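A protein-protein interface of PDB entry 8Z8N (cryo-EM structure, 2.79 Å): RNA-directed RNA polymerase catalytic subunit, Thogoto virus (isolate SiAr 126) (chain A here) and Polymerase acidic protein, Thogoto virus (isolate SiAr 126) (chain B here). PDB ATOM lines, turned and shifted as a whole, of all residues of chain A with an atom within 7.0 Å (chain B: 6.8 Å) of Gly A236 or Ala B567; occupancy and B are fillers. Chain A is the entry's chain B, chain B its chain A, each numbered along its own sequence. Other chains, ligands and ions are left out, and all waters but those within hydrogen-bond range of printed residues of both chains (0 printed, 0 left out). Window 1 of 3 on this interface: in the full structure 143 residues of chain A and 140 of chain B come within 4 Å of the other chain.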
ATOM      1  N   LEU A  19     -20.502   3.125 -14.243  1.00  0.00           N
ATOM      2  CA  LEU A  19     -20.870   2.885 -15.629  1.00  0.00           C
ATOM      3  C   LEU A  19     -20.640   1.440 -16.047  1.00  0.00           C
ATOM      4  O   LEU A  19     -20.484   1.166 -17.241  1.00  0.00           O
ATOM      5  CB  LEU A  19     -20.098   3.827 -16.556  1.00  0.00           C
ATOM      6  CG  LEU A  19     -20.711   5.199 -16.853  1.00  0.00           C
ATOM      7  CD1 LEU A  19     -20.975   5.988 -15.579  1.00  0.00           C
ATOM      8  CD2 LEU A  19     -19.821   5.987 -17.799  1.00  0.00           C
ATOM      9  N   PRO A  27     -24.131 -11.397 -21.557  1.00  0.00           N
ATOM     10  CA  PRO A  27     -24.801 -11.969 -22.729  1.00  0.00           C
ATOM     11  C   PRO A  27     -24.093 -13.210 -23.247  1.00  0.00           C
ATOM     12  O   PRO A  27     -22.866 -13.319 -23.213  1.00  0.00           O
ATOM     13  CB  PRO A  27     -24.748 -10.829 -23.751  1.00  0.00           C
ATOM     14  CG  PRO A  27     -24.708  -9.605 -22.906  1.00  0.00           C
ATOM     15  CD  PRO A  27     -23.820  -9.973 -21.752  1.00  0.00           C
ATOM     16  N   GLU A 234     -18.756 -12.621 -22.637  1.00  0.00           N
ATOM     17  CA  GLU A 234     -18.010 -11.407 -22.925  1.00  0.00           C
ATOM     18  C   GLU A 234     -18.877 -10.186 -22.649  1.00  0.00           C
ATOM     19  O   GLU A 234     -20.092 -10.212 -22.863  1.00  0.00           O
ATOM     20  CB  GLU A 234     -17.531 -11.401 -24.378  1.00  0.00           C
ATOM     21  CG  GLU A 234     -16.500 -10.328 -24.690  1.00  0.00           C
ATOM     22  CD  GLU A 234     -16.160 -10.259 -26.164  1.00  0.00           C
ATOM     23  OE1 GLU A 234     -16.961 -10.755 -26.985  1.00  0.00           O
ATOM     24  OE2 GLU A 234     -15.090  -9.711 -26.504  1.00  0.00           O
ATOM     25  N   ARG A 235     -18.246  -9.116 -22.176  1.00  0.00           N
ATOM     26  CA  ARG A 235     -18.950  -7.919 -21.748  1.00  0.00           C
ATOM     27  C   ARG A 235     -18.422  -6.699 -22.491  1.00  0.00           C
ATOM     28  O   ARG A 235     -17.278  -6.669 -22.952  1.00  0.00           O
ATOM     29  CB  ARG A 235     -18.810  -7.710 -20.235  1.00  0.00           C
ATOM     30  CG  ARG A 235     -19.621  -8.684 -19.399  1.00  0.00           C
ATOM     31  CD  ARG A 235     -19.573  -8.323 -17.925  1.00  0.00           C
ATOM     32  NE  ARG A 235     -20.190  -9.352 -17.098  1.00  0.00           N
ATOM     33  CZ  ARG A 235     -21.458  -9.341 -16.711  1.00  0.00           C
ATOM     34  NH1 ARG A 235     -22.277  -8.361 -17.054  1.00  0.00           N
ATOM     35  NH2 ARG A 235     -21.916 -10.339 -15.961  1.00  0.00           N
ATOM     36  N   GLY A 236     -19.279  -5.687 -22.602  1.00  0.00           N
ATOM     37  CA  GLY A 236     -18.913  -4.434 -23.226  1.00  0.00           C
ATOM     38  C   GLY A 236     -19.136  -4.352 -24.719  1.00  0.00           C
ATOM     39  O   GLY A 236     -18.599  -3.438 -25.354  1.00  0.00           O
ATOM     40  N   ARG A 237     -19.904  -5.269 -25.301  1.00  0.00           N
ATOM     41  CA  ARG A 237     -20.162  -5.273 -26.732  1.00  0.00           C
ATOM     42  C   ARG A 237     -21.644  -5.467 -27.008  1.00  0.00           C
ATOM     43  O   ARG A 237     -22.343  -6.170 -26.277  1.00  0.00           O
ATOM     44  CB  ARG A 237     -19.378  -6.376 -27.448  1.00  0.00           C
ATOM     45  CG  ARG A 237     -17.875  -6.234 -27.379  1.00  0.00           C
ATOM     46  CD  ARG A 237     -17.213  -7.367 -28.135  1.00  0.00           C
ATOM     47  NE  ARG A 237     -17.841  -7.588 -29.433  1.00  0.00           N
ATOM     48  CZ  ARG A 237     -17.516  -6.945 -30.545  1.00  0.00           C
ATOM     49  NH1 ARG A 237     -16.578  -6.013 -30.558  1.00  0.00           N
ATOM     50  NH2 ARG A 237     -18.152  -7.242 -31.675  1.00  0.00           N
ATOM     51  N   LEU A 238     -22.114  -4.843 -28.085  1.00  0.00           N
ATOM     52  CA  LEU A 238     -23.461  -5.093 -28.575  1.00  0.00           C
ATOM     53  C   LEU A 238     -23.527  -6.320 -29.470  1.00  0.00           C
ATOM     54  O   LEU A 238     -24.551  -7.015 -29.488  1.00  0.00           O
ATOM     55  CB  LEU A 238     -23.979  -3.867 -29.336  1.00  0.00           C
ATOM     56  CG  LEU A 238     -25.321  -3.996 -30.060  1.00  0.00           C
ATOM     57  CD1 LEU A 238     -26.476  -3.904 -29.076  1.00  0.00           C
ATOM     58  CD2 LEU A 238     -25.449  -2.940 -31.145  1.00  0.00           C
ATOM     59  N   ASN A 239     -22.452  -6.614 -30.194  1.00  0.00           N
ATOM     60  CA  ASN A 239     -22.392  -7.736 -31.118  1.00  0.00           C
ATOM     61  C   ASN A 239     -21.400  -8.773 -30.610  1.00  0.00           C
ATOM     62  O   ASN A 239     -20.361  -8.427 -30.039  1.00  0.00           O
ATOM     63  CB  ASN A 239     -21.986  -7.267 -32.517  1.00  0.00           C
ATOM     64  CG  ASN A 239     -22.869  -6.151 -33.035  1.00  0.00           C
ATOM     65  OD1 ASN A 239     -22.421  -5.019 -33.206  1.00  0.00           O
ATOM     66  ND2 ASN A 239     -24.134  -6.467 -33.288  1.00  0.00           N
ATOM     67  N   ARG A 240     -21.726 -10.045 -30.820  1.00  0.00           N
ATOM     68  CA  ARG A 240     -20.886 -11.135 -30.349  1.00  0.00           C
ATOM     69  C   ARG A 240     -19.784 -11.429 -31.360  1.00  0.00           C
ATOM     70  O   ARG A 240     -20.029 -11.480 -32.569  1.00  0.00           O
ATOM     71  CB  ARG A 240     -21.727 -12.392 -30.121  1.00  0.00           C
ATOM     72  CG  ARG A 240     -22.875 -12.245 -29.126  1.00  0.00           C
ATOM     73  CD  ARG A 240     -22.413 -12.241 -27.674  1.00  0.00           C
ATOM     74  NE  ARG A 240     -21.814 -10.973 -27.275  1.00  0.00           N
ATOM     75  CZ  ARG A 240     -22.504  -9.874 -27.002  1.00  0.00           C
ATOM     76  NH1 ARG A 240     -23.822  -9.847 -27.092  1.00  0.00           N
ATOM     77  NH2 ARG A 240     -21.854  -8.775 -26.633  1.00  0.00           N
ATOM     78  N   ARG A 241     -18.566 -11.628 -30.863  1.00  0.00           N
ATOM     79  CA  ARG A 241     -17.437 -12.014 -31.698  1.00  0.00           C
ATOM     80  C   ARG A 241     -17.147 -13.503 -31.543  1.00  0.00           C
ATOM     81  O   ARG A 241     -17.707 -14.188 -30.686  1.00  0.00           O
ATOM     82  CB  ARG A 241     -16.178 -11.208 -31.359  1.00  0.00           C
ATOM     83  CG  ARG A 241     -15.607 -11.504 -29.986  1.00  0.00           C
ATOM     84  CD  ARG A 241     -14.415 -10.614 -29.665  1.00  0.00           C
ATOM     85  NE  ARG A 241     -14.740  -9.204 -29.481  1.00  0.00           N
ATOM     86  CZ  ARG A 241     -13.829  -8.251 -29.343  1.00  0.00           C
ATOM     87  NH1 ARG A 241     -12.536  -8.526 -29.364  1.00  0.00           N
ATOM     88  NH2 ARG A 241     -14.222  -6.992 -29.182  1.00  0.00           N
ATOM     89  N   LYS A 458     -13.439   6.130 -31.363  1.00  0.00           N
ATOM     90  CA  LYS A 458     -13.029   5.629 -30.062  1.00  0.00           C
ATOM     91  C   LYS A 458     -11.762   6.280 -29.527  1.00  0.00           C
ATOM     92  O   LYS A 458     -11.451   6.099 -28.344  1.00  0.00           O
ATOM     93  CB  LYS A 458     -12.825   4.109 -30.119  1.00  0.00           C
ATOM     94  CG  LYS A 458     -14.103   3.328 -30.382  1.00  0.00           C
ATOM     95  CD  LYS A 458     -13.983   1.886 -29.927  1.00  0.00           C
ATOM     96  CE  LYS A 458     -15.275   1.127 -30.170  1.00  0.00           C
ATOM     97  NZ  LYS A 458     -15.163  -0.303 -29.772  1.00  0.00           N
ATOM     98  N   GLU A 469      -7.795   6.793 -20.346  1.00  0.00           N
ATOM     99  CA  GLU A 469      -8.066   5.425 -19.930  1.00  0.00           C
ATOM    100  C   GLU A 469      -7.221   4.469 -20.756  1.00  0.00           C
ATOM    101  O   GLU A 469      -6.966   4.713 -21.939  1.00  0.00           O
ATOM    102  CB  GLU A 469      -9.555   5.082 -20.078  1.00  0.00           C
ATOM    103  CG  GLU A 469     -10.063   5.102 -21.511  1.00  0.00           C
ATOM    104  CD  GLU A 469     -11.576   5.161 -21.596  1.00  0.00           C
ATOM    105  OE1 GLU A 469     -12.164   4.346 -22.338  1.00  0.00           O
ATOM    106  OE2 GLU A 469     -12.177   6.025 -20.923  1.00  0.00           O
ATOM    107  N   PRO B 560     -27.028  -7.093 -24.275  1.00  0.00           N
ATOM    108  CA  PRO B 560     -26.008  -6.488 -25.145  1.00  0.00           C
ATOM    109  C   PRO B 560     -26.175  -4.990 -25.317  1.00  0.00           C
ATOM    110  O   PRO B 560     -25.170  -4.270 -25.390  1.00  0.00           O
ATOM    111  CB  PRO B 560     -26.199  -7.237 -26.468  1.00  0.00           C
ATOM    112  CG  PRO B 560     -26.696  -8.567 -26.054  1.00  0.00           C
ATOM    113  CD  PRO B 560     -27.584  -8.323 -24.871  1.00  0.00           C
ATOM    114  N   MET B 562     -27.355  -2.710 -23.123  1.00  0.00           N
ATOM    115  CA  MET B 562     -26.876  -1.973 -21.957  1.00  0.00           C
ATOM    116  C   MET B 562     -25.358  -2.003 -21.858  1.00  0.00           C
ATOM    117  O   MET B 562     -24.724  -0.978 -21.578  1.00  0.00           O
ATOM    118  CB  MET B 562     -27.512  -2.519 -20.677  1.00  0.00           C
ATOM    119  CG  MET B 562     -26.926  -1.905 -19.415  1.00  0.00           C
ATOM    120  SD  MET B 562     -27.665  -0.325 -18.954  1.00  0.00           S
ATOM    121  CE  MET B 562     -29.334  -0.820 -18.561  1.00  0.00           C
ATOM    122  N   GLU B 563     -24.748  -3.171 -22.069  1.00  0.00           N
ATOM    123  CA  GLU B 563     -23.299  -3.240 -21.931  1.00  0.00           C
ATOM    124  C   GLU B 563     -22.601  -2.448 -23.031  1.00  0.00           C
ATOM    125  O   GLU B 563     -21.615  -1.754 -22.765  1.00  0.00           O
ATOM    126  CB  GLU B 563     -22.823  -4.693 -21.912  1.00  0.00           C
ATOM    127  CG  GLU B 563     -23.035  -5.464 -23.188  1.00  0.00           C
ATOM    128  CD  GLU B 563     -22.592  -6.898 -23.051  1.00  0.00           C
ATOM    129  OE1 GLU B 563     -22.148  -7.273 -21.946  1.00  0.00           O
ATOM    130  OE2 GLU B 563     -22.663  -7.645 -24.047  1.00  0.00           O
ATOM    131  N   GLY B 564     -23.106  -2.519 -24.266  1.00  0.00           N
ATOM    132  CA  GLY B 564     -22.540  -1.700 -25.325  1.00  0.00           C
ATOM    133  C   GLY B 564     -22.709  -0.215 -25.062  1.00  0.00           C
ATOM    134  O   GLY B 564     -21.781   0.571 -25.273  1.00  0.00           O
ATOM    135  N   PHE B 565     -23.893   0.183 -24.588  1.00  0.00           N
ATOM    136  CA  PHE B 565     -24.148   1.579 -24.259  1.00  0.00           C
ATOM    137  C   PHE B 565     -23.173   2.079 -23.205  1.00  0.00           C
ATOM    138  O   PHE B 565     -22.559   3.137 -23.365  1.00  0.00           O
ATOM    139  CB  PHE B 565     -25.592   1.730 -23.774  1.00  0.00           C
ATOM    140  CG  PHE B 565     -25.928   3.103 -23.269  1.00  0.00           C
ATOM    141  CD1 PHE B 565     -26.285   4.111 -24.146  1.00  0.00           C
ATOM    142  CD2 PHE B 565     -25.892   3.385 -21.913  1.00  0.00           C
ATOM    143  CE1 PHE B 565     -26.596   5.373 -23.683  1.00  0.00           C
ATOM    144  CE2 PHE B 565     -26.201   4.647 -21.445  1.00  0.00           C
ATOM    145  CZ  PHE B 565     -26.552   5.642 -22.331  1.00  0.00           C
ATOM    146  N   LEU B 566     -23.010   1.321 -22.121  1.00  0.00           N
ATOM    147  CA  LEU B 566     -22.111   1.747 -21.055  1.00  0.00           C
ATOM    148  C   LEU B 566     -20.664   1.781 -21.531  1.00  0.00           C
ATOM    149  O   LEU B 566     -19.934   2.742 -21.249  1.00  0.00           O
ATOM    150  CB  LEU B 566     -22.263   0.824 -19.850  1.00  0.00           C
ATOM    151  CG  LEU B 566     -23.567   0.973 -19.066  1.00  0.00           C
ATOM    152  CD1 LEU B 566     -23.805  -0.247 -18.196  1.00  0.00           C
ATOM    153  CD2 LEU B 566     -23.557   2.242 -18.230  1.00  0.00           C
ATOM    154  N   ALA B 567     -20.236   0.753 -22.268  1.00  0.00           N
ATOM    155  CA  ALA B 567     -18.853   0.690 -22.727  1.00  0.00           C
ATOM    156  C   ALA B 567     -18.525   1.848 -23.656  1.00  0.00           C
ATOM    157  O   ALA B 567     -17.443   2.440 -23.563  1.00  0.00           O
ATOM    158  CB  ALA B 567     -18.594  -0.646 -23.422  1.00  0.00           C
ATOM    159  N   ASN B 568     -19.444   2.192 -24.558  1.00  0.00           N
ATOM    160  CA  ASN B 568     -19.200   3.295 -25.476  1.00  0.00           C
ATOM    161  C   ASN B 568     -19.511   4.657 -24.869  1.00  0.00           C
ATOM    162  O   ASN B 568     -19.125   5.676 -25.452  1.00  0.00           O
ATOM    163  CB  ASN B 568     -20.012   3.090 -26.755  1.00  0.00           C
ATOM    164  CG  ASN B 568     -19.598   1.845 -27.509  1.00  0.00           C
ATOM    165  OD1 ASN B 568     -18.448   1.711 -27.924  1.00  0.00           O
ATOM    166  ND2 ASN B 568     -20.536   0.925 -27.690  1.00  0.00           N
ATOM    167  N   MET B 569     -20.191   4.704 -23.726  1.00  0.00           N
ATOM    168  CA  MET B 569     -20.464   5.955 -23.038  1.00  0.00           C
ATOM    169  C   MET B 569     -19.408   6.302 -22.001  1.00  0.00           C
ATOM    170  O   MET B 569     -19.384   7.442 -21.523  1.00  0.00           O
ATOM    171  CB  MET B 569     -21.837   5.892 -22.359  1.00  0.00           C
ATOM    172  CG  MET B 569     -22.957   6.545 -23.150  1.00  0.00           C
ATOM    173  SD  MET B 569     -22.787   8.335 -23.247  1.00  0.00           S
ATOM    174  CE  MET B 569     -23.104   8.793 -21.550  1.00  0.00           C
ATOM    175  N   ARG B 570     -18.557   5.346 -21.626  1.00  0.00           N
ATOM    176  CA  ARG B 570     -17.469   5.653 -20.701  1.00  0.00           C
ATOM    177  C   ARG B 570     -16.552   6.736 -21.259  1.00  0.00           C
ATOM    178  O   ARG B 570     -16.146   7.653 -20.533  1.00  0.00           O
ATOM    179  CB  ARG B 570     -16.674   4.385 -20.391  1.00  0.00           C
ATOM    180  CG  ARG B 570     -17.482   3.334 -19.664  1.00  0.00           C
ATOM    181  CD  ARG B 570     -16.639   2.414 -18.813  1.00  0.00           C
ATOM    182  NE  ARG B 570     -17.328   1.145 -18.611  1.00  0.00           N
ATOM    183  CZ  ARG B 570     -17.134   0.063 -19.351  1.00  0.00           C
ATOM    184  NH1 ARG B 570     -16.254   0.051 -20.338  1.00  0.00           N
ATOM    185  NH2 ARG B 570     -17.845  -1.032 -19.100  1.00  0.00           N
ATOM    186  N   ARG B 571     -16.218   6.655 -22.549  1.00  0.00           N
ATOM    187  CA  ARG B 571     -15.330   7.654 -23.135  1.00  0.00           C
ATOM    188  C   ARG B 571     -16.003   9.018 -23.241  1.00  0.00           C
ATOM    189  O   ARG B 571     -15.336  10.045 -23.084  1.00  0.00           O
ATOM    190  CB  ARG B 571     -14.828   7.186 -24.501  1.00  0.00           C
ATOM    191  CG  ARG B 571     -15.885   7.096 -25.583  1.00  0.00           C
ATOM    192  CD  ARG B 571     -15.287   6.547 -26.866  1.00  0.00           C
ATOM    193  NE  ARG B 571     -14.739   5.210 -26.676  1.00  0.00           N
ATOM    194  CZ  ARG B 571     -15.374   4.090 -26.989  1.00  0.00           C
ATOM    195  NH1 ARG B 571     -16.583   4.107 -27.525  1.00  0.00           N
ATOM    196  NH2 ARG B 571     -14.781   2.921 -26.760  1.00  0.00           N
ATOM    197  N   LEU B 572     -17.315   9.059 -23.486  1.00  0.00           N
ATOM    198  CA  LEU B 572     -18.011  10.342 -23.493  1.00  0.00           C
ATOM    199  C   LEU B 572     -18.113  10.931 -22.093  1.00  0.00           C
ATOM    200  O   LEU B 572     -18.044  12.154 -21.931  1.00  0.00           O
ATOM    201  CB  LEU B 572     -19.396  10.191 -24.119  1.00  0.00           C
ATOM    202  CG  LEU B 572     -19.386   9.661 -25.553  1.00  0.00           C
ATOM    203  CD1 LEU B 572     -20.786   9.309 -26.018  1.00  0.00           C
ATOM    204  CD2 LEU B 572     -18.749  10.679 -26.481  1.00  0.00           C
ATOM    205  N   VAL B 597     -22.608   4.876 -29.586  1.00  0.00           N
ATOM    206  CA  VAL B 597     -23.579   4.783 -28.502  1.00  0.00           C
ATOM    207  C   VAL B 597     -25.000   4.680 -29.040  1.00  0.00           C
ATOM    208  O   VAL B 597     -25.808   3.901 -28.528  1.00  0.00           O
ATOM    209  CB  VAL B 597     -23.425   5.990 -27.556  1.00  0.00           C
ATOM    210  CG1 VAL B 597     -24.533   5.995 -26.522  1.00  0.00           C
ATOM    211  CG2 VAL B 597     -22.069   5.975 -26.889  1.00  0.00           C
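Among the printed residues, pairs that only touch across the chains: Pro A27 with Glu B563, Leu A19 with Leu B566, Arg A235 with Glu B563, Arg A240 with Pro B560, Gly A236 with Ala B567, Lys A458 with Arg B571, Leu A238 with Pro B560, Arg A237 with Pro B560, Pro A27 with Pro B560, Glu A234 with Glu B563 and Lys A458 with Asn B568.
Of the printed residues of chain B, Glu A234 touches Glu B563 (3.7 Å).
Of the printed residues of chain B, Arg A235 touches Glu B563.
Of chain B, only Glu B563 (3.3 Å) and Ala B567 (3.4 Å) come within 4 Å of Gly A236.
Asn A239 touches none of the printed residues of chain B.
Phe B565 touches none of the printed residues of chain A.
Of the printed residues of chain A, Leu B566 touches Leu A19.
Ala B567 touches one residue of chain A.
Printed residues of chain A within 4 Å of Asn B568: Lys A458 (3.9 Å).
Printed residues of chain A within 4 Å of Arg B570: Leu A19 (3.4 Å).
The nearest residue of chain B that does not touch Gly A236 is Gly B564 (4.3 Å).
The nearest printed residue of chain B that does not touch Lys A458 is Ala B567 (7.1 Å).
ND2 of Asn B568 is in hydrogen-bond range of O of Gly B564, at 2.7 Å.
The backbone carbonyl oxygen (O) of Arg A237 is in hydrogen-bond range of the guanidinium group (NH2) of Arg A240.
The side-chain amide oxygen (OD1) of Asn B568 lies within hydrogen-bond range of the guanidinium group (NH1) of Arg B571 (3.1 Å).
The side-chain carboxylate of Glu A234 is in salt-bridge range of the guanidinium group of Arg A241 (3.0 Å).
The guanidinium group (NE) of Arg A237 lies within hydrogen-bond range of the backbone carbonyl oxygen (O) of Asn A239, 2.7 Å away.
The side-chain carboxylate of Glu B563 is in salt-bridge range of the guanidinium group of Arg A240 (2.9 Å).
O of Arg A237 sits close to OE2 of Glu B563, 2.7 Å away.
N of Gly A236 sits at hydrogen-bond distance from OE1 of Glu B563, at 3.3 Å.
The guanidinium group of Arg B570 is in hydrogen-bond range of the backbone carbonyl oxygen of Leu A19.
Among the printed residues, 15 pairs touch across the chains.
Among the printed residues, Asp or Glu carboxylates within 4 Å of a Lys or Arg side-chain nitrogen of the other chain: Arg A240 with Glu B563 (2.9 Å).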
